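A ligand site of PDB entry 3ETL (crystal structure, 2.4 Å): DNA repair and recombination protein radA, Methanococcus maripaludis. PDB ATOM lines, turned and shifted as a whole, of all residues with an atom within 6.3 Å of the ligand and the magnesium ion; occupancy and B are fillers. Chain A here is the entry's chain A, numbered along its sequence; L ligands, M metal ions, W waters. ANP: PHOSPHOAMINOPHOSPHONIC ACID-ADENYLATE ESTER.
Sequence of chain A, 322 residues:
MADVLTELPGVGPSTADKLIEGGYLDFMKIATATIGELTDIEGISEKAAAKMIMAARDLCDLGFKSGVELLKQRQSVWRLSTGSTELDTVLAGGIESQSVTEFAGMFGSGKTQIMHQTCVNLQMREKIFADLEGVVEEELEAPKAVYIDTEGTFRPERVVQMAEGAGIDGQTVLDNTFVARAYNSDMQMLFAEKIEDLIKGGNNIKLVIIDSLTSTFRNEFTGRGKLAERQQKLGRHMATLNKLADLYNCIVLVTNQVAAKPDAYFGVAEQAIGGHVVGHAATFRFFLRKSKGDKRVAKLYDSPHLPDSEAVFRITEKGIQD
The backbone NH of Thr 112 is in hydrogen-bond range of an oxygen (O1A) of the ligand, 3.0 Å away.
The backbone NH (N) of Lys 111 sits at hydrogen-bond distance from an oxygen (O2B) of the ligand (2.8 Å).
NZ of Lys 111 lies within salt-bridge range of O2B of the ligand, at 2.8 Å.
The backbone NH of Gln 113 sits at hydrogen-bond distance from an oxygen (O1A) of the ligand.
OE1 of Gln 161 lies within hydrogen-bond range of N6 of the ligand, 2.9 Å away.
An oxygen (O2B) of the ligand is in hydrogen-bond range of the backbone NH of Gly 110 (3.1 Å).
OG1 of Thr 112 sits close to OD2 of Asp 211 (3.2 Å).
The side-chain hydroxyl (OG) of Ser 109 sits at hydrogen-bond distance from the side-chain amino group (NZ) of Lys 111, at 3.5 Å.
The side-chain amino group (NZ) of Lys 111 is in hydrogen-bond range of the backbone carbonyl oxygen (O) of Met 106 (2.8 Å).
O of Gly 105 is in hydrogen-bond range of NZ of Lys 111 (3.2 Å).
The guanidinium group (NH2) of Arg 158 lies within hydrogen-bond range of the side-chain amide oxygen (OE1) of Gln 161 (2.9 Å).
O of Glu 317 lies within hydrogen-bond range of NH2 of Arg 158 (3.1 Å).
The side-chain hydroxyl (OG) of Ser 109 sits at hydrogen-bond distance from the backbone carbonyl oxygen (O) of Met 106 (2.8 Å).
O of Ser 109 sits close to NE of Arg 296.
The backbone NH (N) of Gly 108 sits close to a nitrogen (N3B) of the ligand (2.8 Å).
A nitrogen (N6) of the ligand sits close to the guanidinium group of Arg 158.
Residues that only touch the ligand: Ser 109, Phe 107, Thr 316, Gln 257, Glu 317 and Ile 315.
Hydrophobic or aromatic side chains within 4 Å of the ligand: Phe 107 and Ile 315.
Of the 23 residues printed, 13 come within 4 Å of the ligand.
Of the 23 residues printed, 1 comes within 4 Å of the magnesium ion.
The nearest printed residue that does not touch the magnesium ion is Asp 211 (4.3 Å).
The magnesium ion is bound by an oxygen (O1B) of the ligand (2.0 Å), the side-chain hydroxyl of Thr 112 (2.1 Å), water W4 (2.3 Å), water W3 (2.3 Å), water W2 (2.4 Å) and an oxygen (O1G) of the ligand (2.6 Å).
The magnesium ion has six donor atoms within binding distance.
Slightly farther from the magnesium ion lies an oxygen (O2G) of the ligand (2.7 Å).
Water W3 lies within hydrogen-bond range of OG1 of Thr 153 (2.6 Å) and OE1 of Glu 151 (2.7 Å).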
ATOM      1  N   GLY A 105      -7.981  33.732  11.538  1.00  0.00           N
ATOM      2  CA  GLY A 105      -9.171  33.703  10.719  1.00  0.00           C
ATOM      3  C   GLY A 105     -10.327  34.330  11.461  1.00  0.00           C
ATOM      4  O   GLY A 105     -10.216  34.617  12.658  1.00  0.00           O
ATOM      5  N   MET A 106     -11.432  34.555  10.755  1.00  0.00           N
ATOM      6  CA  MET A 106     -12.612  35.165  11.350  1.00  0.00           C
ATOM      7  C   MET A 106     -13.415  34.166  12.174  1.00  0.00           C
ATOM      8  O   MET A 106     -13.016  33.012  12.327  1.00  0.00           O
ATOM      9  CB  MET A 106     -13.487  35.765  10.245  1.00  0.00           C
ATOM     10  CG  MET A 106     -12.741  36.802   9.402  1.00  0.00           C
ATOM     11  SD  MET A 106     -13.771  37.650   8.179  1.00  0.00           S
ATOM     12  CE  MET A 106     -14.213  39.163   9.114  1.00  0.00           C
ATOM     13  N   PHE A 107     -14.548  34.601  12.703  1.00  0.00           N
ATOM     14  CA  PHE A 107     -15.396  33.744  13.525  1.00  0.00           C
ATOM     15  C   PHE A 107     -15.814  32.487  12.771  1.00  0.00           C
ATOM     16  O   PHE A 107     -16.043  32.520  11.564  1.00  0.00           O
ATOM     17  CB  PHE A 107     -16.645  34.504  13.998  1.00  0.00           C
ATOM     18  CG  PHE A 107     -17.771  34.517  12.984  1.00  0.00           C
ATOM     19  CD1 PHE A 107     -18.657  33.441  12.872  1.00  0.00           C
ATOM     20  CD2 PHE A 107     -17.945  35.608  12.127  1.00  0.00           C
ATOM     21  CE1 PHE A 107     -19.692  33.436  11.929  1.00  0.00           C
ATOM     22  CE2 PHE A 107     -18.979  35.616  11.179  1.00  0.00           C
ATOM     23  CZ  PHE A 107     -19.849  34.531  11.083  1.00  0.00           C
ATOM     24  N   GLY A 108     -15.918  31.383  13.499  1.00  0.00           N
ATOM     25  CA  GLY A 108     -16.339  30.126  12.905  1.00  0.00           C
ATOM     26  C   GLY A 108     -15.555  29.594  11.738  1.00  0.00           C
ATOM     27  O   GLY A 108     -16.019  28.682  11.061  1.00  0.00           O
ATOM     28  N   SER A 109     -14.373  30.137  11.485  1.00  0.00           N
ATOM     29  CA  SER A 109     -13.587  29.637  10.362  1.00  0.00           C
ATOM     30  C   SER A 109     -13.042  28.239  10.644  1.00  0.00           C
ATOM     31  O   SER A 109     -12.680  27.510   9.709  1.00  0.00           O
ATOM     32  CB  SER A 109     -12.469  30.623   9.983  1.00  0.00           C
ATOM     33  OG  SER A 109     -11.631  30.947  11.078  1.00  0.00           O
ATOM     34  N   GLY A 110     -12.983  27.851  11.914  1.00  0.00           N
ATOM     35  CA  GLY A 110     -12.521  26.515  12.268  1.00  0.00           C
ATOM     36  C   GLY A 110     -11.186  26.390  12.993  1.00  0.00           C
ATOM     37  O   GLY A 110     -10.558  25.319  12.979  1.00  0.00           O
ATOM     38  N   LYS A 111     -10.739  27.476  13.612  1.00  0.00           N
ATOM     39  CA  LYS A 111      -9.486  27.518  14.344  1.00  0.00           C
ATOM     40  C   LYS A 111      -9.508  26.546  15.525  1.00  0.00           C
ATOM     41  O   LYS A 111      -8.555  25.782  15.721  1.00  0.00           O
ATOM     42  CB  LYS A 111      -9.242  28.937  14.870  1.00  0.00           C
ATOM     43  CG  LYS A 111      -9.237  30.021  13.808  1.00  0.00           C
ATOM     44  CD  LYS A 111      -8.909  31.395  14.410  1.00  0.00           C
ATOM     45  CE  LYS A 111     -10.084  31.958  15.206  1.00  0.00           C
ATOM     46  NZ  LYS A 111     -11.296  32.067  14.331  1.00  0.00           N
ATOM     47  N   THR A 112     -10.589  26.582  16.299  1.00  0.00           N
ATOM     48  CA  THR A 112     -10.750  25.724  17.467  1.00  0.00           C
ATOM     49  C   THR A 112     -10.896  24.249  17.094  1.00  0.00           C
ATOM     50  O   THR A 112     -10.359  23.385  17.782  1.00  0.00           O
ATOM     51  CB  THR A 112     -11.976  26.183  18.328  1.00  0.00           C
ATOM     52  OG1 THR A 112     -11.762  27.528  18.796  1.00  0.00           O
ATOM     53  CG2 THR A 112     -12.143  25.269  19.547  1.00  0.00           C
ATOM     54  N   GLN A 113     -11.624  23.970  16.016  1.00  0.00           N
ATOM     55  CA  GLN A 113     -11.810  22.604  15.550  1.00  0.00           C
ATOM     56  C   GLN A 113     -10.462  21.957  15.278  1.00  0.00           C
ATOM     57  O   GLN A 113     -10.217  20.804  15.620  1.00  0.00           O
ATOM     58  CB  GLN A 113     -12.649  22.579  14.264  1.00  0.00           C
ATOM     59  CG  GLN A 113     -14.085  23.024  14.464  1.00  0.00           C
ATOM     60  CD  GLN A 113     -14.743  22.341  15.667  1.00  0.00           C
ATOM     61  OE1 GLN A 113     -14.990  21.137  15.640  1.00  0.00           O
ATOM     62  NE2 GLN A 113     -15.020  23.113  16.718  1.00  0.00           N
ATOM     63  N   ILE A 114      -9.576  22.718  14.644  1.00  0.00           N
ATOM     64  CA  ILE A 114      -8.258  22.207  14.311  1.00  0.00           C
ATOM     65  C   ILE A 114      -7.448  21.927  15.569  1.00  0.00           C
ATOM     66  O   ILE A 114      -6.704  20.963  15.636  1.00  0.00           O
ATOM     67  CB  ILE A 114      -7.490  23.187  13.396  1.00  0.00           C
ATOM     68  CG1 ILE A 114      -8.144  23.202  12.010  1.00  0.00           C
ATOM     69  CG2 ILE A 114      -6.014  22.809  13.317  1.00  0.00           C
ATOM     70  CD1 ILE A 114      -7.464  24.138  11.040  1.00  0.00           C
ATOM     71  N   GLU A 151     -10.830  31.430  26.014  1.00  0.00           N
ATOM     72  CA  GLU A 151     -12.193  31.934  25.883  1.00  0.00           C
ATOM     73  C   GLU A 151     -13.175  30.950  26.466  1.00  0.00           C
ATOM     74  O   GLU A 151     -14.369  31.216  26.542  1.00  0.00           O
ATOM     75  CB  GLU A 151     -12.507  32.174  24.404  1.00  0.00           C
ATOM     76  CG  GLU A 151     -11.535  33.139  23.766  1.00  0.00           C
ATOM     77  CD  GLU A 151     -11.372  32.893  22.288  1.00  0.00           C
ATOM     78  OE1 GLU A 151     -11.093  31.727  21.924  1.00  0.00           O
ATOM     79  OE2 GLU A 151     -11.507  33.851  21.498  1.00  0.00           O
ATOM     80  N   THR A 153     -13.668  27.717  25.247  1.00  0.00           N
ATOM     81  CA  THR A 153     -14.311  26.967  24.176  1.00  0.00           C
ATOM     82  C   THR A 153     -13.901  25.490  24.110  1.00  0.00           C
ATOM     83  O   THR A 153     -14.382  24.748  23.259  1.00  0.00           O
ATOM     84  CB  THR A 153     -14.042  27.588  22.774  1.00  0.00           C
ATOM     85  OG1 THR A 153     -12.634  27.721  22.568  1.00  0.00           O
ATOM     86  CG2 THR A 153     -14.718  28.935  22.661  1.00  0.00           C
ATOM     87  N   ARG A 158     -16.312  17.088  22.079  1.00  0.00           N
ATOM     88  CA  ARG A 158     -15.917  17.222  20.681  1.00  0.00           C
ATOM     89  C   ARG A 158     -14.663  16.396  20.436  1.00  0.00           C
ATOM     90  O   ARG A 158     -14.472  15.834  19.364  1.00  0.00           O
ATOM     91  CB  ARG A 158     -15.717  18.706  20.346  1.00  0.00           C
ATOM     92  CG  ARG A 158     -15.405  19.003  18.903  1.00  0.00           C
ATOM     93  CD  ARG A 158     -16.412  18.393  17.937  1.00  0.00           C
ATOM     94  NE  ARG A 158     -16.122  18.793  16.567  1.00  0.00           N
ATOM     95  CZ  ARG A 158     -16.348  18.035  15.506  1.00  0.00           C
ATOM     96  NH1 ARG A 158     -16.050  18.499  14.290  1.00  0.00           N
ATOM     97  NH2 ARG A 158     -16.856  16.817  15.633  1.00  0.00           N
ATOM     98  N   GLN A 161     -15.743  12.783  20.342  1.00  0.00           N
ATOM     99  CA  GLN A 161     -16.418  12.558  19.082  1.00  0.00           C
ATOM    100  C   GLN A 161     -15.404  12.440  17.927  1.00  0.00           C
ATOM    101  O   GLN A 161     -15.547  11.582  17.061  1.00  0.00           O
ATOM    102  CB  GLN A 161     -17.404  13.707  18.830  1.00  0.00           C
ATOM    103  CG  GLN A 161     -18.118  13.681  17.517  1.00  0.00           C
ATOM    104  CD  GLN A 161     -19.073  14.864  17.375  1.00  0.00           C
ATOM    105  OE1 GLN A 161     -18.740  15.996  17.715  1.00  0.00           O
ATOM    106  NE2 GLN A 161     -20.264  14.595  16.842  1.00  0.00           N
ATOM    107  N   ASP A 211      -5.271  28.689  22.677  1.00  0.00           N
ATOM    108  CA  ASP A 211      -6.495  29.063  21.986  1.00  0.00           C
ATOM    109  C   ASP A 211      -7.368  29.961  22.884  1.00  0.00           C
ATOM    110  O   ASP A 211      -8.030  29.462  23.790  1.00  0.00           O
ATOM    111  CB  ASP A 211      -7.257  27.774  21.623  1.00  0.00           C
ATOM    112  CG  ASP A 211      -8.540  28.024  20.845  1.00  0.00           C
ATOM    113  OD1 ASP A 211      -8.567  28.938  19.995  1.00  0.00           O
ATOM    114  OD2 ASP A 211      -9.523  27.302  21.079  1.00  0.00           O
ATOM    115  N   THR A 255      -3.980  30.234  18.007  1.00  0.00           N
ATOM    116  CA  THR A 255      -5.052  30.751  17.173  1.00  0.00           C
ATOM    117  C   THR A 255      -5.119  32.251  17.394  1.00  0.00           C
ATOM    118  O   THR A 255      -4.746  32.767  18.449  1.00  0.00           O
ATOM    119  CB  THR A 255      -6.420  30.136  17.519  1.00  0.00           C
ATOM    120  OG1 THR A 255      -6.812  30.526  18.845  1.00  0.00           O
ATOM    121  CG2 THR A 255      -6.363  28.620  17.397  1.00  0.00           C
ATOM    122  N   GLN A 257      -7.813  35.621  16.420  1.00  0.00           N
ATOM    123  CA  GLN A 257      -9.043  36.062  15.791  1.00  0.00           C
ATOM    124  C   GLN A 257      -8.734  37.382  15.113  1.00  0.00           C
ATOM    125  O   GLN A 257      -7.976  38.185  15.632  1.00  0.00           O
ATOM    126  CB  GLN A 257     -10.159  36.263  16.807  1.00  0.00           C
ATOM    127  CG  GLN A 257     -11.548  36.030  16.174  1.00  0.00           C
ATOM    128  CD  GLN A 257     -12.678  36.701  16.954  1.00  0.00           C
ATOM    129  OE1 GLN A 257     -13.797  36.201  16.974  1.00  0.00           O
ATOM    130  NE2 GLN A 257     -12.374  37.838  17.571  1.00  0.00           N
ATOM    131  N   LEU A 288      -7.577  31.321   7.697  1.00  0.00           N
ATOM    132  CA  LEU A 288      -8.645  30.344   7.529  1.00  0.00           C
ATOM    133  C   LEU A 288      -9.910  31.063   7.081  1.00  0.00           C
ATOM    134  O   LEU A 288     -10.234  32.125   7.613  1.00  0.00           O
ATOM    135  CB  LEU A 288      -8.911  29.631   8.867  1.00  0.00           C
ATOM    136  CG  LEU A 288      -8.478  28.157   9.051  1.00  0.00           C
ATOM    137  CD1 LEU A 288      -7.022  27.991   8.709  1.00  0.00           C
ATOM    138  CD2 LEU A 288      -8.746  27.745  10.487  1.00  0.00           C
ATOM    139  N   ARG A 296     -13.766  24.544   3.960  1.00  0.00           N
ATOM    140  CA  ARG A 296     -12.928  25.565   4.555  1.00  0.00           C
ATOM    141  C   ARG A 296     -11.686  25.693   3.691  1.00  0.00           C
ATOM    142  O   ARG A 296     -11.339  24.773   2.951  1.00  0.00           O
ATOM    143  CB  ARG A 296     -12.514  25.160   5.976  1.00  0.00           C
ATOM    144  CG  ARG A 296     -13.660  25.011   6.962  1.00  0.00           C
ATOM    145  CD  ARG A 296     -14.156  26.363   7.429  1.00  0.00           C
ATOM    146  NE  ARG A 296     -15.207  26.247   8.443  1.00  0.00           N
ATOM    147  CZ  ARG A 296     -16.427  25.792   8.202  1.00  0.00           C
ATOM    148  NH1 ARG A 296     -16.767  25.387   6.976  1.00  0.00           N
ATOM    149  NH2 ARG A 296     -17.315  25.727   9.188  1.00  0.00           N
ATOM    150  N   ILE A 315     -15.006  20.254   7.756  1.00  0.00           N
ATOM    151  CA  ILE A 315     -15.253  20.087   9.180  1.00  0.00           C
ATOM    152  C   ILE A 315     -16.555  19.284   9.225  1.00  0.00           C
ATOM    153  O   ILE A 315     -17.555  19.700   8.642  1.00  0.00           O
ATOM    154  CB  ILE A 315     -15.493  21.415   9.920  1.00  0.00           C
ATOM    155  CG1 ILE A 315     -14.283  22.347   9.780  1.00  0.00           C
ATOM    156  CG2 ILE A 315     -15.776  21.148  11.382  1.00  0.00           C
ATOM    157  CD1 ILE A 315     -13.089  21.934  10.609  1.00  0.00           C
ATOM    158  N   THR A 316     -16.534  18.140   9.902  1.00  0.00           N
ATOM    159  CA  THR A 316     -17.704  17.272  10.010  1.00  0.00           C
ATOM    160  C   THR A 316     -17.753  16.593  11.373  1.00  0.00           C
ATOM    161  O   THR A 316     -16.872  16.761  12.210  1.00  0.00           O
ATOM    162  CB  THR A 316     -17.672  16.160   8.944  1.00  0.00           C
ATOM    163  OG1 THR A 316     -16.543  15.307   9.199  1.00  0.00           O
ATOM    164  CG2 THR A 316     -17.543  16.731   7.533  1.00  0.00           C
ATOM    165  N   GLU A 317     -18.801  15.802  11.585  1.00  0.00           N
ATOM    166  CA  GLU A 317     -18.972  15.066  12.818  1.00  0.00           C
ATOM    167  C   GLU A 317     -17.707  14.271  13.122  1.00  0.00           C
ATOM    168  O   GLU A 317     -17.349  14.071  14.282  1.00  0.00           O
ATOM    169  CB  GLU A 317     -20.197  14.133  12.712  1.00  0.00           C
ATOM    170  CG  GLU A 317     -20.731  13.920  11.278  1.00  0.00           C
ATOM    171  CD  GLU A 317     -19.986  12.833  10.484  1.00  0.00           C
ATOM    172  OE1 GLU A 317     -20.108  11.634  10.834  1.00  0.00           O
ATOM    173  OE2 GLU A 317     -19.273  13.181   9.515  1.00  0.00           O
ATOM    174  N   LYS A 318     -17.021  13.809  12.085  1.00  0.00           N
ATOM    175  CA  LYS A 318     -15.787  13.072  12.282  1.00  0.00           C
ATOM    176  C   LYS A 318     -14.704  14.035  12.738  1.00  0.00           C
ATOM    177  O   LYS A 318     -13.873  13.700  13.560  1.00  0.00           O
ATOM    178  CB  LYS A 318     -15.349  12.381  10.980  1.00  0.00           C
ATOM    179  CG  LYS A 318     -16.030  11.047  10.755  1.00  0.00           C
ATOM    180  CD  LYS A 318     -15.597  10.365   9.456  1.00  0.00           C
ATOM    181  CE  LYS A 318     -14.123   9.967   9.464  1.00  0.00           C
ATOM    182  NZ  LYS A 318     -13.721   9.322   8.183  1.00  0.00           N
HETATM  183  PG  ANP L   1     -14.280  31.530  17.083  1.00  0.00           P
HETATM  184  O1G ANP L   1     -12.965  31.793  17.535  1.00  0.00           O
HETATM  185  O2G ANP L   1     -14.977  30.661  18.072  1.00  0.00           O
HETATM  186  O3G ANP L   1     -15.013  32.771  16.969  1.00  0.00           O
HETATM  187  PB  ANP L   1     -13.520  29.363  15.372  1.00  0.00           P
HETATM  188  O1B ANP L   1     -12.918  28.848  16.631  1.00  0.00           O
HETATM  189  O2B ANP L   1     -12.468  29.569  14.397  1.00  0.00           O
HETATM  190  N3B ANP L   1     -14.239  30.754  15.602  1.00  0.00           N
HETATM  191  PA  ANP L   1     -14.779  26.795  15.393  1.00  0.00           P
HETATM  192  O1A ANP L   1     -13.425  26.086  15.502  1.00  0.00           O
HETATM  193  O2A ANP L   1     -15.380  26.910  16.735  1.00  0.00           O
HETATM  194  O3A ANP L   1     -14.571  28.287  14.753  1.00  0.00           O
HETATM  195  O5' ANP L   1     -15.759  25.896  14.399  1.00  0.00           O
HETATM  196  C5' ANP L   1     -17.207  26.278  14.143  1.00  0.00           C
HETATM  197  C4' ANP L   1     -17.755  25.441  13.243  1.00  0.00           C
HETATM  198  O4' ANP L   1     -17.352  24.046  13.559  1.00  0.00           O
HETATM  199  C3' ANP L   1     -19.301  25.415  13.456  1.00  0.00           C
HETATM  200  O3' ANP L   1     -19.970  26.579  13.153  1.00  0.00           O
HETATM  201  C2' ANP L   1     -19.758  23.969  13.087  1.00  0.00           C
HETATM  202  O2' ANP L   1     -20.296  23.955  11.641  1.00  0.00           O
HETATM  203  C1' ANP L   1     -18.453  23.149  13.183  1.00  0.00           C
HETATM  204  N9  ANP L   1     -18.637  22.190  14.118  1.00  0.00           N
HETATM  205  C8  ANP L   1     -18.374  22.274  15.496  1.00  0.00           C
HETATM  206  N7  ANP L   1     -18.691  21.162  16.066  1.00  0.00           N
HETATM  207  C5  ANP L   1     -19.150  20.311  15.126  1.00  0.00           C
HETATM  208  C6  ANP L   1     -19.628  19.001  15.163  1.00  0.00           C
HETATM  209  N6  ANP L   1     -19.694  18.335  16.337  1.00  0.00           N
HETATM  210  N1  ANP L   1     -20.041  18.392  13.959  1.00  0.00           N
HETATM  211  C2  ANP L   1     -19.980  19.088  12.726  1.00  0.00           C
HETATM  212  N3  ANP L   1     -19.528  20.373  12.661  1.00  0.00           N
HETATM  213  C4  ANP L   1     -19.117  20.944  13.904  1.00  0.00           C
HETATM  214 MG    MG M   1     -12.556  29.446  18.518  1.00  0.00          MG
HETATM  215  O   HOH W   1     -10.896  33.080  18.755  1.00  0.00           O
HETATM  216  O   HOH W   2     -10.328  30.225  18.407  1.00  0.00           O
HETATM  217  O   HOH W   3     -12.415  29.619  20.828  1.00  0.00           O
HETATM  218  O   HOH W   4     -14.463  28.236  18.860  1.00  0.00           O
